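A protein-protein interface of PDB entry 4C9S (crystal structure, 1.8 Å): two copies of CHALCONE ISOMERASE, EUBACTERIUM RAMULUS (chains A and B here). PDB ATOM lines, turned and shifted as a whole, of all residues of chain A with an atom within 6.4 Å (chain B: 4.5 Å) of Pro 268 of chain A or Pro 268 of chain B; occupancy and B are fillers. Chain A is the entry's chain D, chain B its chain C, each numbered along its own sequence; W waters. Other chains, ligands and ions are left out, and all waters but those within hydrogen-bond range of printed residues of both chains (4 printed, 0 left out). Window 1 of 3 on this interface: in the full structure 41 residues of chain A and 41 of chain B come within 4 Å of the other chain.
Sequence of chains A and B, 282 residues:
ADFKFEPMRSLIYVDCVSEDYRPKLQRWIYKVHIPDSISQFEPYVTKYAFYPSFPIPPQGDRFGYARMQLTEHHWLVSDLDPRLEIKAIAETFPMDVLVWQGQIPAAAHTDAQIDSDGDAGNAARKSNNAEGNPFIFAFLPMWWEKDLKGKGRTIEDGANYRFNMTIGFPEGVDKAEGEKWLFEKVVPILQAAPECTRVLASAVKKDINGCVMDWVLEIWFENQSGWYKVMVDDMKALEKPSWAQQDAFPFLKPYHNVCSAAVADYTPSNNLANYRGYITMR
ND2 of Asn 274 of chain B sits close to O of Asn 274 of chain A, at 3.5 Å.
The backbone carbonyl oxygen (O) of Ser 269 of chain A sits at hydrogen-bond distance from the backbone NH (N) of Phe 50 of chain A. The backbone carbonyl oxygen (O) of Ser 269 of chain A lies close to the side-chain amide oxygen (OD1) of Asn 271 of chain A, 3.5 Å away. The side-chain hydroxyl (OG1) of Thr 267 of chain B is in hydrogen-bond range of the backbone NH (N) of Ser 269 of chain B (3.0 Å). The side-chain amide nitrogen (ND2) of Asn 274 of chain B is in hydrogen-bond range of the backbone carbonyl oxygen (O) of Pro 268 of chain B, 3.0 Å away. OH of Tyr 30 of chain A is in hydrogen-bond range of OG of Ser 269 of chain A (3.1 Å). The side-chain hydroxyl of Thr 267 of chain A lies within hydrogen-bond range of the backbone NH of Ser 269 of chain A (2.9 Å).
CD2 of Tyr 30 of chain A touches CE2 of Tyr 266 of chain B, 3.5 Å away. Pro 268 of chain A touches Pro 268 of chain B. Pro 268 of chain A touches Ser 269 of chain B. Ser 269 of chain A touches Pro 268 of chain B.
Of the printed residues of chain B, Tyr 30 of chain A touches Tyr 266 (3.5 Å). Of the printed residues of chain B, Pro 268 of chain A touches Pro 268 and Ser 269. Printed residues of chain B within 4 Å of Ser 269 of chain A: Pro 268 (3.5 Å). Of chain A, only Pro 268 and Ser 269 come within 4 Å of Pro 268 of chain B. The nearest printed residue of chain B that does not touch Tyr 30 of chain A is Pro 268 of chain B (4.7 Å).
Of the 10 printed residues of chain A, 4 touch a printed residue of chain B. Of the 6 printed residues of chain B, 4 touch a printed residue of chain A. Printed residues of chain B that touch a printed residue of chain A: Tyr 266, Pro 268, Ser 269 and Asn 274. Among the printed residues, 5 pairs touch across the chains. Among the printed residues, no Asp or Glu carboxylate lies within 4 Å of a Lys or Arg side-chain nitrogen of the other chain.
Pro 268 of chain A touches its own counterpart, Pro 268 of chain B. Pro 268 of chain A touches Ser 269 of chain B, and with the chains exchanged Ser 269 of chain A touches Pro 268 of chain B. Asn 274 of chain A touches its own counterpart, Asn 274 of chain B. Of the 5 pairs that touch across the chains among the printed residues, 4 have their exchanged pair printed and touching as well.
Water W4 bridges the backbone carbonyl oxygen (O) of Pro 268 of chain A and the backbone carbonyl oxygen (O) of Pro 268 of chain B. Water W2 lies within hydrogen-bond range of OH of Tyr 266 of chain B (2.8 Å) and O of Asn 274 of chain A (3.3 Å). Water W1 bridges the backbone carbonyl oxygen of Asn 274 of chain B (3.0 Å) and the side-chain amide oxygen of Asn 274 of chain A (3.4 Å). Water W3 lies within hydrogen-bond range of the backbone carbonyl oxygen (O) of Asn 274 of chain A (3.2 Å) and the side-chain amide oxygen (OD1) of Asn 274 of chain B (3.3 Å).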
ATOM      1  N   TYR A  30      34.866 -16.915 -12.268  1.00  0.00           N
ATOM      2  CA  TYR A  30      34.838 -16.400 -13.654  1.00  0.00           C
ATOM      3  C   TYR A  30      36.064 -15.621 -14.135  1.00  0.00           C
ATOM      4  O   TYR A  30      36.317 -15.559 -15.350  1.00  0.00           O
ATOM      5  CB  TYR A  30      33.593 -15.582 -13.871  1.00  0.00           C
ATOM      6  CG  TYR A  30      32.355 -16.490 -13.967  1.00  0.00           C
ATOM      7  CD1 TYR A  30      31.662 -16.889 -12.831  1.00  0.00           C
ATOM      8  CD2 TYR A  30      31.962 -16.998 -15.176  1.00  0.00           C
ATOM      9  CE1 TYR A  30      30.543 -17.712 -12.913  1.00  0.00           C
ATOM     10  CE2 TYR A  30      30.859 -17.832 -15.288  1.00  0.00           C
ATOM     11  CZ  TYR A  30      30.157 -18.188 -14.197  1.00  0.00           C
ATOM     12  OH  TYR A  30      29.092 -19.022 -14.235  1.00  0.00           O
ATOM     13  N   PHE A  50      29.640 -24.542 -16.334  1.00  0.00           N
ATOM     14  CA  PHE A  50      29.092 -24.239 -15.000  1.00  0.00           C
ATOM     15  C   PHE A  50      27.574 -24.123 -15.139  1.00  0.00           C
ATOM     16  O   PHE A  50      27.075 -23.436 -16.030  1.00  0.00           O
ATOM     17  CB  PHE A  50      29.558 -22.909 -14.454  1.00  0.00           C
ATOM     18  CG  PHE A  50      31.065 -22.721 -14.412  1.00  0.00           C
ATOM     19  CD1 PHE A  50      31.908 -23.772 -14.205  1.00  0.00           C
ATOM     20  CD2 PHE A  50      31.578 -21.449 -14.462  1.00  0.00           C
ATOM     21  CE1 PHE A  50      33.267 -23.596 -14.087  1.00  0.00           C
ATOM     22  CE2 PHE A  50      32.939 -21.252 -14.350  1.00  0.00           C
ATOM     23  CZ  PHE A  50      33.787 -22.323 -14.147  1.00  0.00           C
ATOM     24  N   PRO A  52      24.643 -22.741 -12.891  1.00  0.00           N
ATOM     25  CA  PRO A  52      24.373 -22.065 -11.630  1.00  0.00           C
ATOM     26  C   PRO A  52      23.152 -22.658 -10.964  1.00  0.00           C
ATOM     27  O   PRO A  52      22.162 -22.995 -11.632  1.00  0.00           O
ATOM     28  CB  PRO A  52      24.060 -20.596 -12.030  1.00  0.00           C
ATOM     29  CG  PRO A  52      24.269 -20.525 -13.470  1.00  0.00           C
ATOM     30  CD  PRO A  52      24.609 -21.863 -14.057  1.00  0.00           C
ATOM     31  N   TYR A 266      19.695 -25.163 -19.561  1.00  0.00           N
ATOM     32  CA  TYR A 266      20.658 -24.457 -20.339  1.00  0.00           C
ATOM     33  C   TYR A 266      21.520 -23.633 -19.430  1.00  0.00           C
ATOM     34  O   TYR A 266      21.042 -23.097 -18.425  1.00  0.00           O
ATOM     35  CB  TYR A 266      19.925 -23.470 -21.282  1.00  0.00           C
ATOM     36  CG  TYR A 266      20.794 -22.424 -21.948  1.00  0.00           C
ATOM     37  CD1 TYR A 266      21.578 -22.741 -23.065  1.00  0.00           C
ATOM     38  CD2 TYR A 266      20.893 -21.134 -21.458  1.00  0.00           C
ATOM     39  CE1 TYR A 266      22.401 -21.806 -23.667  1.00  0.00           C
ATOM     40  CE2 TYR A 266      21.724 -20.165 -22.054  1.00  0.00           C
ATOM     41  CZ  TYR A 266      22.453 -20.509 -23.177  1.00  0.00           C
ATOM     42  OH  TYR A 266      23.314 -19.658 -23.823  1.00  0.00           O
ATOM     43  N   THR A 267      22.808 -23.571 -19.758  1.00  0.00           N
ATOM     44  CA  THR A 267      23.696 -22.559 -19.163  1.00  0.00           C
ATOM     45  C   THR A 267      24.373 -21.683 -20.219  1.00  0.00           C
ATOM     46  O   THR A 267      24.874 -22.178 -21.226  1.00  0.00           O
ATOM     47  CB  THR A 267      24.771 -23.171 -18.255  1.00  0.00           C
ATOM     48  OG1 THR A 267      25.516 -22.100 -17.641  1.00  0.00           O
ATOM     49  CG2 THR A 267      25.707 -24.074 -19.042  1.00  0.00           C
ATOM     50  N   PRO A 268      24.487 -20.374 -19.958  1.00  0.00           N
ATOM     51  CA  PRO A 268      25.349 -19.555 -20.799  1.00  0.00           C
ATOM     52  C   PRO A 268      26.815 -19.804 -20.548  1.00  0.00           C
ATOM     53  O   PRO A 268      27.629 -19.410 -21.362  1.00  0.00           O
ATOM     54  CB  PRO A 268      25.010 -18.118 -20.416  1.00  0.00           C
ATOM     55  CG  PRO A 268      24.473 -18.241 -19.076  1.00  0.00           C
ATOM     56  CD  PRO A 268      23.820 -19.599 -18.902  1.00  0.00           C
ATOM     57  N   SER A 269      27.155 -20.497 -19.474  1.00  0.00           N
ATOM     58  CA  SER A 269      28.557 -20.717 -19.151  1.00  0.00           C
ATOM     59  C   SER A 269      29.096 -22.046 -19.690  1.00  0.00           C
ATOM     60  O   SER A 269      29.492 -22.941 -18.942  1.00  0.00           O
ATOM     61  CB  SER A 269      28.736 -20.599 -17.636  1.00  0.00           C
ATOM     62  OG  SER A 269      28.472 -19.274 -17.234  1.00  0.00           O
ATOM     63  N   ASN A 270      29.194 -22.097 -21.011  1.00  0.00           N
ATOM     64  CA  ASN A 270      29.798 -23.207 -21.697  1.00  0.00           C
ATOM     65  C   ASN A 270      31.163 -22.738 -22.072  1.00  0.00           C
ATOM     66  O   ASN A 270      31.389 -22.107 -23.115  1.00  0.00           O
ATOM     67  CB  ASN A 270      28.961 -23.669 -22.911  1.00  0.00           C
ATOM     68  CG  ASN A 270      29.460 -24.986 -23.462  1.00  0.00           C
ATOM     69  OD1 ASN A 270      29.999 -25.838 -22.722  1.00  0.00           O
ATOM     70  ND2 ASN A 270      29.296 -25.167 -24.782  1.00  0.00           N
ATOM     71  N   ASN A 271      32.081 -22.994 -21.162  1.00  0.00           N
ATOM     72  CA  ASN A 271      33.283 -22.140 -21.076  1.00  0.00           C
ATOM     73  C   ASN A 271      34.257 -22.303 -22.251  1.00  0.00           C
ATOM     74  O   ASN A 271      34.897 -21.340 -22.612  1.00  0.00           O
ATOM     75  CB  ASN A 271      34.005 -22.331 -19.762  1.00  0.00           C
ATOM     76  CG  ASN A 271      33.097 -21.994 -18.584  1.00  0.00           C
ATOM     77  OD1 ASN A 271      32.343 -21.013 -18.654  1.00  0.00           O
ATOM     78  ND2 ASN A 271      33.191 -22.763 -17.505  1.00  0.00           N
ATOM     79  N   ASN A 274      32.337 -20.167 -25.047  1.00  0.00           N
ATOM     80  CA  ASN A 274      31.566 -18.920 -24.796  1.00  0.00           C
ATOM     81  C   ASN A 274      32.376 -17.861 -24.037  1.00  0.00           C
ATOM     82  O   ASN A 274      31.911 -16.708 -23.900  1.00  0.00           O
ATOM     83  CB  ASN A 274      30.248 -19.195 -24.020  1.00  0.00           C
ATOM     84  CG  ASN A 274      29.216 -20.048 -24.847  1.00  0.00           C
ATOM     85  OD1 ASN A 274      29.504 -20.501 -25.969  1.00  0.00           O
ATOM     86  ND2 ASN A 274      28.043 -20.286 -24.277  1.00  0.00           N
ATOM     87  N   TYR B 266      30.392  -9.036 -13.761  1.00  0.00           N
ATOM     88  CA  TYR B 266      30.507  -9.822 -15.010  1.00  0.00           C
ATOM     89  C   TYR B 266      29.233 -10.636 -15.255  1.00  0.00           C
ATOM     90  O   TYR B 266      28.660 -11.141 -14.324  1.00  0.00           O
ATOM     91  CB  TYR B 266      31.696 -10.785 -14.899  1.00  0.00           C
ATOM     92  CG  TYR B 266      31.767 -11.805 -15.993  1.00  0.00           C
ATOM     93  CD1 TYR B 266      32.291 -11.466 -17.242  1.00  0.00           C
ATOM     94  CD2 TYR B 266      31.254 -13.096 -15.824  1.00  0.00           C
ATOM     95  CE1 TYR B 266      32.392 -12.436 -18.239  1.00  0.00           C
ATOM     96  CE2 TYR B 266      31.309 -14.038 -16.836  1.00  0.00           C
ATOM     97  CZ  TYR B 266      31.910 -13.700 -18.044  1.00  0.00           C
ATOM     98  OH  TYR B 266      31.978 -14.605 -19.089  1.00  0.00           O
ATOM     99  N   THR B 267      28.827 -10.715 -16.517  1.00  0.00           N
ATOM    100  CA  THR B 267      27.819 -11.666 -16.948  1.00  0.00           C
ATOM    101  C   THR B 267      28.320 -12.568 -18.036  1.00  0.00           C
ATOM    102  O   THR B 267      28.919 -12.101 -18.983  1.00  0.00           O
ATOM    103  CB  THR B 267      26.519 -11.025 -17.377  1.00  0.00           C
ATOM    104  OG1 THR B 267      25.581 -12.084 -17.675  1.00  0.00           O
ATOM    105  CG2 THR B 267      26.653 -10.083 -18.599  1.00  0.00           C
ATOM    106  N   PRO B 268      27.974 -13.862 -17.969  1.00  0.00           N
ATOM    107  CA  PRO B 268      28.247 -14.651 -19.164  1.00  0.00           C
ATOM    108  C   PRO B 268      27.319 -14.397 -20.352  1.00  0.00           C
ATOM    109  O   PRO B 268      27.606 -14.841 -21.465  1.00  0.00           O
ATOM    110  CB  PRO B 268      28.140 -16.080 -18.693  1.00  0.00           C
ATOM    111  CG  PRO B 268      27.203 -16.028 -17.558  1.00  0.00           C
ATOM    112  CD  PRO B 268      27.482 -14.677 -16.849  1.00  0.00           C
ATOM    113  N   SER B 269      26.182 -13.763 -20.092  1.00  0.00           N
ATOM    114  CA  SER B 269      25.148 -13.516 -21.061  1.00  0.00           C
ATOM    115  C   SER B 269      25.344 -12.185 -21.757  1.00  0.00           C
ATOM    116  O   SER B 269      24.521 -11.287 -21.637  1.00  0.00           O
ATOM    117  CB  SER B 269      23.779 -13.620 -20.388  1.00  0.00           C
ATOM    118  OG  SER B 269      23.591 -14.965 -19.969  1.00  0.00           O
ATOM    119  N   ASN B 270      26.448 -12.089 -22.507  1.00  0.00           N
ATOM    120  CA  ASN B 270      26.727 -10.988 -23.398  1.00  0.00           C
ATOM    121  C   ASN B 270      26.305 -11.505 -24.767  1.00  0.00           C
ATOM    122  O   ASN B 270      27.049 -12.163 -25.493  1.00  0.00           O
ATOM    123  CB  ASN B 270      28.205 -10.553 -23.325  1.00  0.00           C
ATOM    124  CG  ASN B 270      28.446  -9.244 -24.096  1.00  0.00           C
ATOM    125  OD1 ASN B 270      27.539  -8.404 -24.180  1.00  0.00           O
ATOM    126  ND2 ASN B 270      29.624  -9.086 -24.647  1.00  0.00           N
ATOM    127  N   ASN B 274      28.166 -14.018 -27.389  1.00  0.00           N
ATOM    128  CA  ASN B 274      28.393 -15.293 -26.660  1.00  0.00           C
ATOM    129  C   ASN B 274      27.298 -16.353 -26.944  1.00  0.00           C
ATOM    130  O   ASN B 274      27.486 -17.561 -26.639  1.00  0.00           O
ATOM    131  CB  ASN B 274      28.447 -15.086 -25.132  1.00  0.00           C
ATOM    132  CG  ASN B 274      29.640 -14.232 -24.661  1.00  0.00           C
ATOM    133  OD1 ASN B 274      30.474 -13.751 -25.460  1.00  0.00           O
ATOM    134  ND2 ASN B 274      29.717 -14.040 -23.367  1.00  0.00           N
HETATM  135  O   HOH W   1      30.074 -18.009 -28.152  1.00  0.00           O
HETATM  136  O   HOH W   2      31.101 -16.800 -20.664  1.00  0.00           O
HETATM  137  O   HOH W   3      31.975 -16.223 -27.105  1.00  0.00           O
HETATM  138  O   HOH W   4      27.179 -17.181 -22.859  1.00  0.00           O
